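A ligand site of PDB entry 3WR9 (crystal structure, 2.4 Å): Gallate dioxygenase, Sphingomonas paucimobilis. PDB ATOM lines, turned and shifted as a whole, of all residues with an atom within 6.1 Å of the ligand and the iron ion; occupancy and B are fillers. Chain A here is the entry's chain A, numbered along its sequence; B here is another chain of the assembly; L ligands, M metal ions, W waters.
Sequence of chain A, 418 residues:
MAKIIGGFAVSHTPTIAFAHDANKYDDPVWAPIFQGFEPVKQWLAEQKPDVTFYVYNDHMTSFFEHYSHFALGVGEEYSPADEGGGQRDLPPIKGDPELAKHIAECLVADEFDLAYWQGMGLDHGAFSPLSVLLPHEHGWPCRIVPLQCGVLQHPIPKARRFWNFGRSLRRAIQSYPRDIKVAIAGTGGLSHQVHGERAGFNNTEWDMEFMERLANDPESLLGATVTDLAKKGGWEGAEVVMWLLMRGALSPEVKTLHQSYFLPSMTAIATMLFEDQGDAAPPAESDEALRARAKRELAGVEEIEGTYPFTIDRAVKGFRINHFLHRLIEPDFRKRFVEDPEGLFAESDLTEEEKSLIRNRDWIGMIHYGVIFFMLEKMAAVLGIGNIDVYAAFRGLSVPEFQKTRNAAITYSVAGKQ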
ATOM      1  N   HIS A  12       2.138  23.536   1.587  1.00  0.00           N
ATOM      2  CA  HIS A  12       1.719  22.912   2.858  1.00  0.00           C
ATOM      3  C   HIS A  12       0.252  22.454   2.895  1.00  0.00           C
ATOM      4  O   HIS A  12      -0.340  22.274   3.963  1.00  0.00           O
ATOM      5  CB  HIS A  12       2.072  23.772   4.096  1.00  0.00           C
ATOM      6  CG  HIS A  12       1.385  25.112   4.169  1.00  0.00           C
ATOM      7  ND1 HIS A  12       2.054  26.252   4.590  1.00  0.00           N
ATOM      8  CD2 HIS A  12       0.111  25.489   3.929  1.00  0.00           C
ATOM      9  CE1 HIS A  12       1.205  27.270   4.603  1.00  0.00           C
ATOM     10  NE2 HIS A  12       0.022  26.837   4.188  1.00  0.00           N
ATOM     11  N   THR A  13      -0.342  22.299   1.715  1.00  0.00           N
ATOM     12  CA  THR A  13      -1.748  21.888   1.638  1.00  0.00           C
ATOM     13  C   THR A  13      -1.977  20.568   2.357  1.00  0.00           C
ATOM     14  O   THR A  13      -1.153  19.674   2.277  1.00  0.00           O
ATOM     15  CB  THR A  13      -2.222  21.763   0.179  1.00  0.00           C
ATOM     16  OG1 THR A  13      -3.481  21.065   0.157  1.00  0.00           O
ATOM     17  CG2 THR A  13      -1.180  21.056  -0.734  1.00  0.00           C
ATOM     18  N   PRO A  14      -3.099  20.463   3.093  1.00  0.00           N
ATOM     19  CA  PRO A  14      -3.500  19.228   3.804  1.00  0.00           C
ATOM     20  C   PRO A  14      -3.769  18.051   2.846  1.00  0.00           C
ATOM     21  O   PRO A  14      -4.064  16.944   3.295  1.00  0.00           O
ATOM     22  CB  PRO A  14      -4.761  19.645   4.547  1.00  0.00           C
ATOM     23  CG  PRO A  14      -5.258  20.877   3.784  1.00  0.00           C
ATOM     24  CD  PRO A  14      -4.037  21.573   3.346  1.00  0.00           C
ATOM     25  N   THR A  15      -3.645  18.271   1.547  1.00  0.00           N
ATOM     26  CA  THR A  15      -3.613  17.171   0.581  1.00  0.00           C
ATOM     27  C   THR A  15      -2.400  16.284   0.828  1.00  0.00           C
ATOM     28  O   THR A  15      -2.432  15.073   0.545  1.00  0.00           O
ATOM     29  CB  THR A  15      -3.466  17.727  -0.845  1.00  0.00           C
ATOM     30  OG1 THR A  15      -4.584  18.567  -1.135  1.00  0.00           O
ATOM     31  CG2 THR A  15      -3.400  16.602  -1.880  1.00  0.00           C
ATOM     32  N   ASN A  57       2.481  29.479   8.131  1.00  0.00           N
ATOM     33  CA  ASN A  57       1.384  30.200   8.721  1.00  0.00           C
ATOM     34  C   ASN A  57       0.387  29.212   9.346  1.00  0.00           C
ATOM     35  O   ASN A  57       0.154  28.130   8.804  1.00  0.00           O
ATOM     36  CB  ASN A  57       0.734  31.145   7.703  1.00  0.00           C
ATOM     37  CG  ASN A  57      -0.183  30.424   6.747  1.00  0.00           C
ATOM     38  OD1 ASN A  57       0.246  29.780   5.794  1.00  0.00           O
ATOM     39  ND2 ASN A  57      -1.477  30.546   6.995  1.00  0.00           N
ATOM     40  N   HIS A  59      -3.344  28.254  10.282  1.00  0.00           N
ATOM     41  CA  HIS A  59      -4.577  28.545   9.544  1.00  0.00           C
ATOM     42  C   HIS A  59      -5.750  28.735  10.515  1.00  0.00           C
ATOM     43  O   HIS A  59      -6.706  27.966  10.537  1.00  0.00           O
ATOM     44  CB  HIS A  59      -4.802  27.486   8.462  1.00  0.00           C
ATOM     45  CG  HIS A  59      -3.708  27.433   7.440  1.00  0.00           C
ATOM     46  ND1 HIS A  59      -2.453  26.927   7.716  1.00  0.00           N
ATOM     47  CD2 HIS A  59      -3.662  27.888   6.163  1.00  0.00           C
ATOM     48  CE1 HIS A  59      -1.684  27.065   6.656  1.00  0.00           C
ATOM     49  NE2 HIS A  59      -2.389  27.635   5.694  1.00  0.00           N
ATOM     50  N   HIS A 124      -1.578  22.069  10.085  1.00  0.00           N
ATOM     51  CA  HIS A 124      -1.137  21.559   8.787  1.00  0.00           C
ATOM     52  C   HIS A 124      -0.134  22.478   8.072  1.00  0.00           C
ATOM     53  O   HIS A 124       0.659  22.011   7.246  1.00  0.00           O
ATOM     54  CB  HIS A 124      -2.355  21.220   7.903  1.00  0.00           C
ATOM     55  CG  HIS A 124      -3.014  22.417   7.247  1.00  0.00           C
ATOM     56  ND1 HIS A 124      -4.206  22.951   7.704  1.00  0.00           N
ATOM     57  CD2 HIS A 124      -2.667  23.127   6.144  1.00  0.00           C
ATOM     58  CE1 HIS A 124      -4.556  23.950   6.907  1.00  0.00           C
ATOM     59  NE2 HIS A 124      -3.637  24.082   5.957  1.00  0.00           N
ATOM     60  N   GLY A 125      -0.173  23.769   8.398  1.00  0.00           N
ATOM     61  CA  GLY A 125       0.823  24.718   7.890  1.00  0.00           C
ATOM     62  C   GLY A 125       2.235  24.189   8.099  1.00  0.00           C
ATOM     63  O   GLY A 125       3.136  24.400   7.264  1.00  0.00           O
ATOM     64  N   GLY A 188       3.888  27.006   2.076  1.00  0.00           N
ATOM     65  CA  GLY A 188       2.669  27.624   1.523  1.00  0.00           C
ATOM     66  C   GLY A 188       2.696  27.592  -0.003  1.00  0.00           C
ATOM     67  O   GLY A 188       3.679  27.141  -0.591  1.00  0.00           O
ATOM     68  N   GLY A 189       1.623  28.046  -0.649  1.00  0.00           N
ATOM     69  CA  GLY A 189       1.640  28.114  -2.122  1.00  0.00           C
ATOM     70  C   GLY A 189       1.507  26.776  -2.853  1.00  0.00           C
ATOM     71  O   GLY A 189       1.221  25.755  -2.230  1.00  0.00           O
ATOM     72  N   HIS A 192      -3.433  29.074  -5.420  1.00  0.00           N
ATOM     73  CA  HIS A 192      -4.680  28.474  -5.005  1.00  0.00           C
ATOM     74  C   HIS A 192      -5.640  29.528  -4.429  1.00  0.00           C
ATOM     75  O   HIS A 192      -5.206  30.565  -3.901  1.00  0.00           O
ATOM     76  CB  HIS A 192      -4.468  27.319  -4.011  1.00  0.00           C
ATOM     77  CG  HIS A 192      -3.883  27.740  -2.683  1.00  0.00           C
ATOM     78  ND1 HIS A 192      -2.636  28.315  -2.553  1.00  0.00           N
ATOM     79  CD2 HIS A 192      -4.359  27.580  -1.414  1.00  0.00           C
ATOM     80  CE1 HIS A 192      -2.386  28.535  -1.272  1.00  0.00           C
ATOM     81  NE2 HIS A 192      -3.409  28.087  -0.555  1.00  0.00           N
ATOM     82  N   VAL A 194      -9.194  29.124  -1.920  1.00  0.00           N
ATOM     83  CA  VAL A 194     -10.007  28.142  -1.231  1.00  0.00           C
ATOM     84  C   VAL A 194     -11.235  28.794  -0.587  1.00  0.00           C
ATOM     85  O   VAL A 194     -11.932  28.161   0.213  1.00  0.00           O
ATOM     86  CB  VAL A 194      -9.160  27.336  -0.176  1.00  0.00           C
ATOM     87  CG1 VAL A 194      -8.157  26.412  -0.869  1.00  0.00           C
ATOM     88  CG2 VAL A 194      -8.418  28.243   0.792  1.00  0.00           C
ATOM     89  N   GLU A 236      -5.310  32.987  -1.435  1.00  0.00           N
ATOM     90  CA  GLU A 236      -4.412  32.344  -0.471  1.00  0.00           C
ATOM     91  C   GLU A 236      -3.024  32.102  -1.061  1.00  0.00           C
ATOM     92  O   GLU A 236      -2.020  32.051  -0.332  1.00  0.00           O
ATOM     93  CB  GLU A 236      -5.021  31.073   0.116  1.00  0.00           C
ATOM     94  CG  GLU A 236      -6.235  31.316   1.025  1.00  0.00           C
ATOM     95  CD  GLU A 236      -7.531  31.700   0.282  1.00  0.00           C
ATOM     96  OE1 GLU A 236      -7.625  31.507  -0.956  1.00  0.00           O
ATOM     97  OE2 GLU A 236      -8.462  32.203   0.936  1.00  0.00           O
ATOM     98  N   GLU A 239       0.316  33.899   0.027  1.00  0.00           N
ATOM     99  CA  GLU A 239       1.107  33.496   1.206  1.00  0.00           C
ATOM    100  C   GLU A 239       2.576  33.226   0.827  1.00  0.00           C
ATOM    101  O   GLU A 239       3.434  33.049   1.704  1.00  0.00           O
ATOM    102  CB  GLU A 239       0.473  32.285   1.911  1.00  0.00           C
ATOM    103  CG  GLU A 239       0.666  30.923   1.231  1.00  0.00           C
ATOM    104  CD  GLU A 239      -0.169  29.802   1.876  1.00  0.00           C
ATOM    105  OE1 GLU A 239      -0.666  29.982   2.994  1.00  0.00           O
ATOM    106  OE2 GLU A 239      -0.340  28.727   1.257  1.00  0.00           O
ATOM    107  N   SER A 265      -5.347  18.901  -7.591  1.00  0.00           N
ATOM    108  CA  SER A 265      -6.631  19.386  -7.151  1.00  0.00           C
ATOM    109  C   SER A 265      -6.665  20.911  -7.021  1.00  0.00           C
ATOM    110  O   SER A 265      -6.600  21.603  -8.033  1.00  0.00           O
ATOM    111  CB  SER A 265      -7.028  18.666  -5.871  1.00  0.00           C
ATOM    112  OG  SER A 265      -8.389  18.881  -5.561  1.00  0.00           O
ATOM    113  N   MET A 266      -6.718  21.451  -5.800  1.00  0.00           N
ATOM    114  CA  MET A 266      -6.963  22.884  -5.578  1.00  0.00           C
ATOM    115  C   MET A 266      -5.694  23.706  -5.582  1.00  0.00           C
ATOM    116  O   MET A 266      -5.689  24.863  -6.028  1.00  0.00           O
ATOM    117  CB  MET A 266      -7.690  23.094  -4.245  1.00  0.00           C
ATOM    118  CG  MET A 266      -9.073  22.541  -4.239  1.00  0.00           C
ATOM    119  SD  MET A 266     -10.263  23.532  -5.187  1.00  0.00           S
ATOM    120  CE  MET A 266     -10.338  25.072  -4.278  1.00  0.00           C
ATOM    121  N   THR A 267      -4.630  23.116  -5.079  1.00  0.00           N
ATOM    122  CA  THR A 267      -3.365  23.821  -4.904  1.00  0.00           C
ATOM    123  C   THR A 267      -2.257  23.344  -5.853  1.00  0.00           C
ATOM    124  O   THR A 267      -2.121  22.139  -6.127  1.00  0.00           O
ATOM    125  CB  THR A 267      -2.879  23.722  -3.432  1.00  0.00           C
ATOM    126  OG1 THR A 267      -3.937  24.136  -2.542  1.00  0.00           O
ATOM    127  CG2 THR A 267      -1.661  24.596  -3.223  1.00  0.00           C
ATOM    128  N   PHE B 373     -12.617  30.907   5.721  1.00  0.00           N
ATOM    129  CA  PHE B 373     -12.747  29.537   5.247  1.00  0.00           C
ATOM    130  C   PHE B 373     -12.223  28.527   6.273  1.00  0.00           C
ATOM    131  O   PHE B 373     -12.812  27.469   6.470  1.00  0.00           O
ATOM    132  CB  PHE B 373     -12.016  29.327   3.928  1.00  0.00           C
ATOM    133  CG  PHE B 373     -11.754  27.874   3.605  1.00  0.00           C
ATOM    134  CD1 PHE B 373     -12.808  27.021   3.258  1.00  0.00           C
ATOM    135  CD2 PHE B 373     -10.456  27.352   3.662  1.00  0.00           C
ATOM    136  CE1 PHE B 373     -12.560  25.655   2.968  1.00  0.00           C
ATOM    137  CE2 PHE B 373     -10.200  26.004   3.369  1.00  0.00           C
ATOM    138  CZ  PHE B 373     -11.258  25.142   3.024  1.00  0.00           C
ATOM    139  N   PHE B 374     -11.114  28.836   6.917  1.00  0.00           N
ATOM    140  CA  PHE B 374     -10.524  27.856   7.813  1.00  0.00           C
ATOM    141  C   PHE B 374     -11.432  27.439   8.961  1.00  0.00           C
ATOM    142  O   PHE B 374     -11.315  26.311   9.444  1.00  0.00           O
ATOM    143  CB  PHE B 374      -9.108  28.263   8.212  1.00  0.00           C
ATOM    144  CG  PHE B 374      -8.265  28.605   7.024  1.00  0.00           C
ATOM    145  CD1 PHE B 374      -7.701  27.598   6.262  1.00  0.00           C
ATOM    146  CD2 PHE B 374      -8.087  29.924   6.630  1.00  0.00           C
ATOM    147  CE1 PHE B 374      -6.939  27.908   5.151  1.00  0.00           C
ATOM    148  CE2 PHE B 374      -7.346  30.243   5.517  1.00  0.00           C
ATOM    149  CZ  PHE B 374      -6.774  29.245   4.767  1.00  0.00           C
ATOM    150  N   GLU B 377     -13.398  24.817   7.069  1.00  0.00           N
ATOM    151  CA  GLU B 377     -12.537  23.645   6.928  1.00  0.00           C
ATOM    152  C   GLU B 377     -12.649  22.715   8.141  1.00  0.00           C
ATOM    153  O   GLU B 377     -12.739  21.492   7.985  1.00  0.00           O
ATOM    154  CB  GLU B 377     -11.073  24.093   6.730  1.00  0.00           C
ATOM    155  CG  GLU B 377     -10.089  22.979   6.361  1.00  0.00           C
ATOM    156  CD  GLU B 377      -8.679  23.496   6.089  1.00  0.00           C
ATOM    157  OE1 GLU B 377      -8.100  24.228   6.945  1.00  0.00           O
ATOM    158  OE2 GLU B 377      -8.120  23.172   5.006  1.00  0.00           O
ATOM    159  N   ASN B 387     -12.984  18.821   2.160  1.00  0.00           N
ATOM    160  CA  ASN B 387     -12.806  20.173   1.603  1.00  0.00           C
ATOM    161  C   ASN B 387     -13.519  20.365   0.256  1.00  0.00           C
ATOM    162  O   ASN B 387     -14.183  21.394   0.052  1.00  0.00           O
ATOM    163  CB  ASN B 387     -11.308  20.525   1.454  1.00  0.00           C
ATOM    164  CG  ASN B 387     -10.571  20.617   2.785  1.00  0.00           C
ATOM    165  OD1 ASN B 387     -10.781  19.808   3.686  1.00  0.00           O
ATOM    166  ND2 ASN B 387      -9.669  21.602   2.894  1.00  0.00           N
ATOM    167  N   TYR B 391     -15.760  23.535  -1.344  1.00  0.00           N
ATOM    168  CA  TYR B 391     -15.424  24.245  -2.569  1.00  0.00           C
ATOM    169  C   TYR B 391     -16.530  24.146  -3.599  1.00  0.00           C
ATOM    170  O   TYR B 391     -16.898  25.157  -4.199  1.00  0.00           O
ATOM    171  CB  TYR B 391     -14.093  23.752  -3.170  1.00  0.00           C
ATOM    172  CG  TYR B 391     -12.960  23.725  -2.176  1.00  0.00           C
ATOM    173  CD1 TYR B 391     -12.783  24.780  -1.279  1.00  0.00           C
ATOM    174  CD2 TYR B 391     -12.041  22.660  -2.151  1.00  0.00           C
ATOM    175  CE1 TYR B 391     -11.739  24.770  -0.369  1.00  0.00           C
ATOM    176  CE2 TYR B 391     -10.965  22.647  -1.236  1.00  0.00           C
ATOM    177  CZ  TYR B 391     -10.832  23.699  -0.348  1.00  0.00           C
ATOM    178  OH  TYR B 391      -9.818  23.736   0.577  1.00  0.00           O
ATOM    179  N   TYR B 412      -9.753  14.919   0.312  1.00  0.00           N
ATOM    180  CA  TYR B 412      -8.869  15.076   1.459  1.00  0.00           C
ATOM    181  C   TYR B 412      -9.539  15.910   2.556  1.00  0.00           C
ATOM    182  O   TYR B 412     -10.568  16.544   2.323  1.00  0.00           O
ATOM    183  CB  TYR B 412      -7.529  15.711   1.030  1.00  0.00           C
ATOM    184  CG  TYR B 412      -7.668  17.030   0.271  1.00  0.00           C
ATOM    185  CD1 TYR B 412      -7.781  17.054  -1.133  1.00  0.00           C
ATOM    186  CD2 TYR B 412      -7.692  18.253   0.954  1.00  0.00           C
ATOM    187  CE1 TYR B 412      -7.926  18.252  -1.830  1.00  0.00           C
ATOM    188  CE2 TYR B 412      -7.833  19.464   0.278  1.00  0.00           C
ATOM    189  CZ  TYR B 412      -7.954  19.448  -1.116  1.00  0.00           C
ATOM    190  OH  TYR B 412      -8.075  20.629  -1.783  1.00  0.00           O
ATOM    191  N   VAL B 414      -8.595  17.903   6.824  1.00  0.00           N
ATOM    192  CA  VAL B 414      -7.618  18.214   7.869  1.00  0.00           C
ATOM    193  C   VAL B 414      -7.733  17.239   9.060  1.00  0.00           C
ATOM    194  O   VAL B 414      -7.140  17.487  10.115  1.00  0.00           O
ATOM    195  CB  VAL B 414      -7.735  19.686   8.385  1.00  0.00           C
ATOM    196  CG1 VAL B 414      -7.225  20.664   7.350  1.00  0.00           C
ATOM    197  CG2 VAL B 414      -9.172  20.026   8.813  1.00  0.00           C
HETATM  198  O1  LIG L   1      -7.523  22.751  -0.164  1.00  0.00           O
HETATM  199  O2  LIG L   1      -5.629  22.708  -1.310  1.00  0.00           O
HETATM  200  O3  LIG L   1      -2.564  25.734   1.478  1.00  0.00           O
HETATM  201  O4  LIG L   1      -6.339  24.754   4.219  1.00  0.00           O
HETATM  202  O5  LIG L   1      -3.793  25.994   3.924  1.00  0.00           O
HETATM  203  C1  LIG L   1      -4.400  24.471   0.636  1.00  0.00           C
HETATM  204  C2  LIG L   1      -6.280  24.003   2.025  1.00  0.00           C
HETATM  205  C3  LIG L   1      -6.315  23.087  -0.308  1.00  0.00           C
HETATM  206  C4  LIG L   1      -3.785  25.169   1.673  1.00  0.00           C
HETATM  207  C5  LIG L   1      -5.669  24.691   3.064  1.00  0.00           C
HETATM  208  C6  LIG L   1      -5.649  23.882   0.802  1.00  0.00           C
HETATM  209  C7  LIG L   1      -4.420  25.293   2.905  1.00  0.00           C
HETATM  210 FE    FE M   1      -2.373  27.248   3.459  1.00  0.00          FE
HETATM  211  O   HOH W   1      -2.669  30.054   4.415  1.00  0.00           O
HETATM  212  O   HOH W   2      -5.090  20.508  -3.419  1.00  0.00           O
HETATM  213  O   HOH W   3       0.000  25.092   0.073  1.00  0.00           O
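The backbone NH (N) of Asn 387 of chain B is in hydrogen-bond range of the backbone carbonyl oxygen (O) of Tyr 412 of chain B.
OH of Tyr 391 of chain B lies within hydrogen-bond range of ND2 of Asn 387 of chain B.
N of Gly 188 is in hydrogen-bond range of ND1 of His 12 (3.2 Å).
NE2 of His 12 sits close to OE1 of Glu 239 (3.4 Å).
The side-chain carboxylate (OE2) of Glu 239 sits at hydrogen-bond distance from the backbone NH (N) of Gly 189 (2.8 Å).
The side-chain amide oxygen (OD1) of Asn 57 lies close to a ring nitrogen (NE2) of His 12, 3.4 Å away.
The side-chain hydroxyl (OG1) of Thr 15 lies within hydrogen-bond range of the side-chain hydroxyl (OG1) of Thr 13, at 3.0 Å.
ND1 of His 59 lies close to O of Asn 57 (3.1 Å).
Merely in contact with the iron ion: Glu 239 (3.3 Å).
Pro 14 touches the ligand.
Val 194 touches the ligand (CG1 to O1, 3.8 Å).
OE2 of Glu 239 touches O3 of the ligand, 3.7 Å away.
Met 266 touches the ligand.
Phe 374 of chain B touches the ligand (CE1 to O4, 3.3 Å).
ND2 of Asn 387 of chain B touches O1 of the ligand (3.9 Å).
Hydrophobic or aromatic side chains that line the ligand: His 12, Pro 14, His 59, His 124, His 192, Val 194, Met 266, Phe 374 of chain B, Tyr 391 of chain B and Tyr 412 of chain B.
Of the 24 residues printed, 15 come within 4 Å of the ligand.
The nearest printed residue that does not touch the ligand is Phe 373 of chain B (4.1 Å).
Water W1 bridges OE1 of Glu 239 (2.5 Å) and ND2 of Asn 57 (2.9 Å).
Water W3 lies within hydrogen-bond range of the backbone carbonyl oxygen of Gly 189, the backbone NH of His 12 and the backbone NH of Thr 13.
Water W2 lies within hydrogen-bond range of the backbone NH (N) of Met 266 (3.0 Å), the side-chain hydroxyl (OG1) of Thr 15 (3.0 Å), an oxygen (O2) of the ligand (3.1 Å), the backbone NH (N) of Thr 267 (3.1 Å) and the side-chain hydroxyl (OH) of Tyr 412 of chain B (3.4 Å).
O2 of the ligand sits at hydrogen-bond distance from OG1 of Thr 267, 2.5 Å away.
NE2 of His 192 sits close to O3 of the ligand, at 3.2 Å.
The side-chain hydroxyl of Tyr 412 of chain B lies within hydrogen-bond range of an oxygen (O1) of the ligand.
The side-chain hydroxyl (OH) of Tyr 391 of chain B is in hydrogen-bond range of an oxygen (O1) of the ligand, 2.6 Å away.
NE2 of His 124 is in hydrogen-bond range of O4 of the ligand (3.3 Å).
An oxygen (O4) of the ligand lies within hydrogen-bond range of the side-chain carboxylate (OE2) of Glu 377 of chain B, 2.5 Å away.
OG1 of Thr 13 lies within hydrogen-bond range of O2 of the ligand.
The iron ion is bound by O5 of the ligand (2.0 Å).
The iron ion is bound by NE2 of His 59, at 2.3 Å.
O3 of the ligand binds the iron ion (2.5 Å).
NE2 of His 12 binds the iron ion (2.5 Å).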
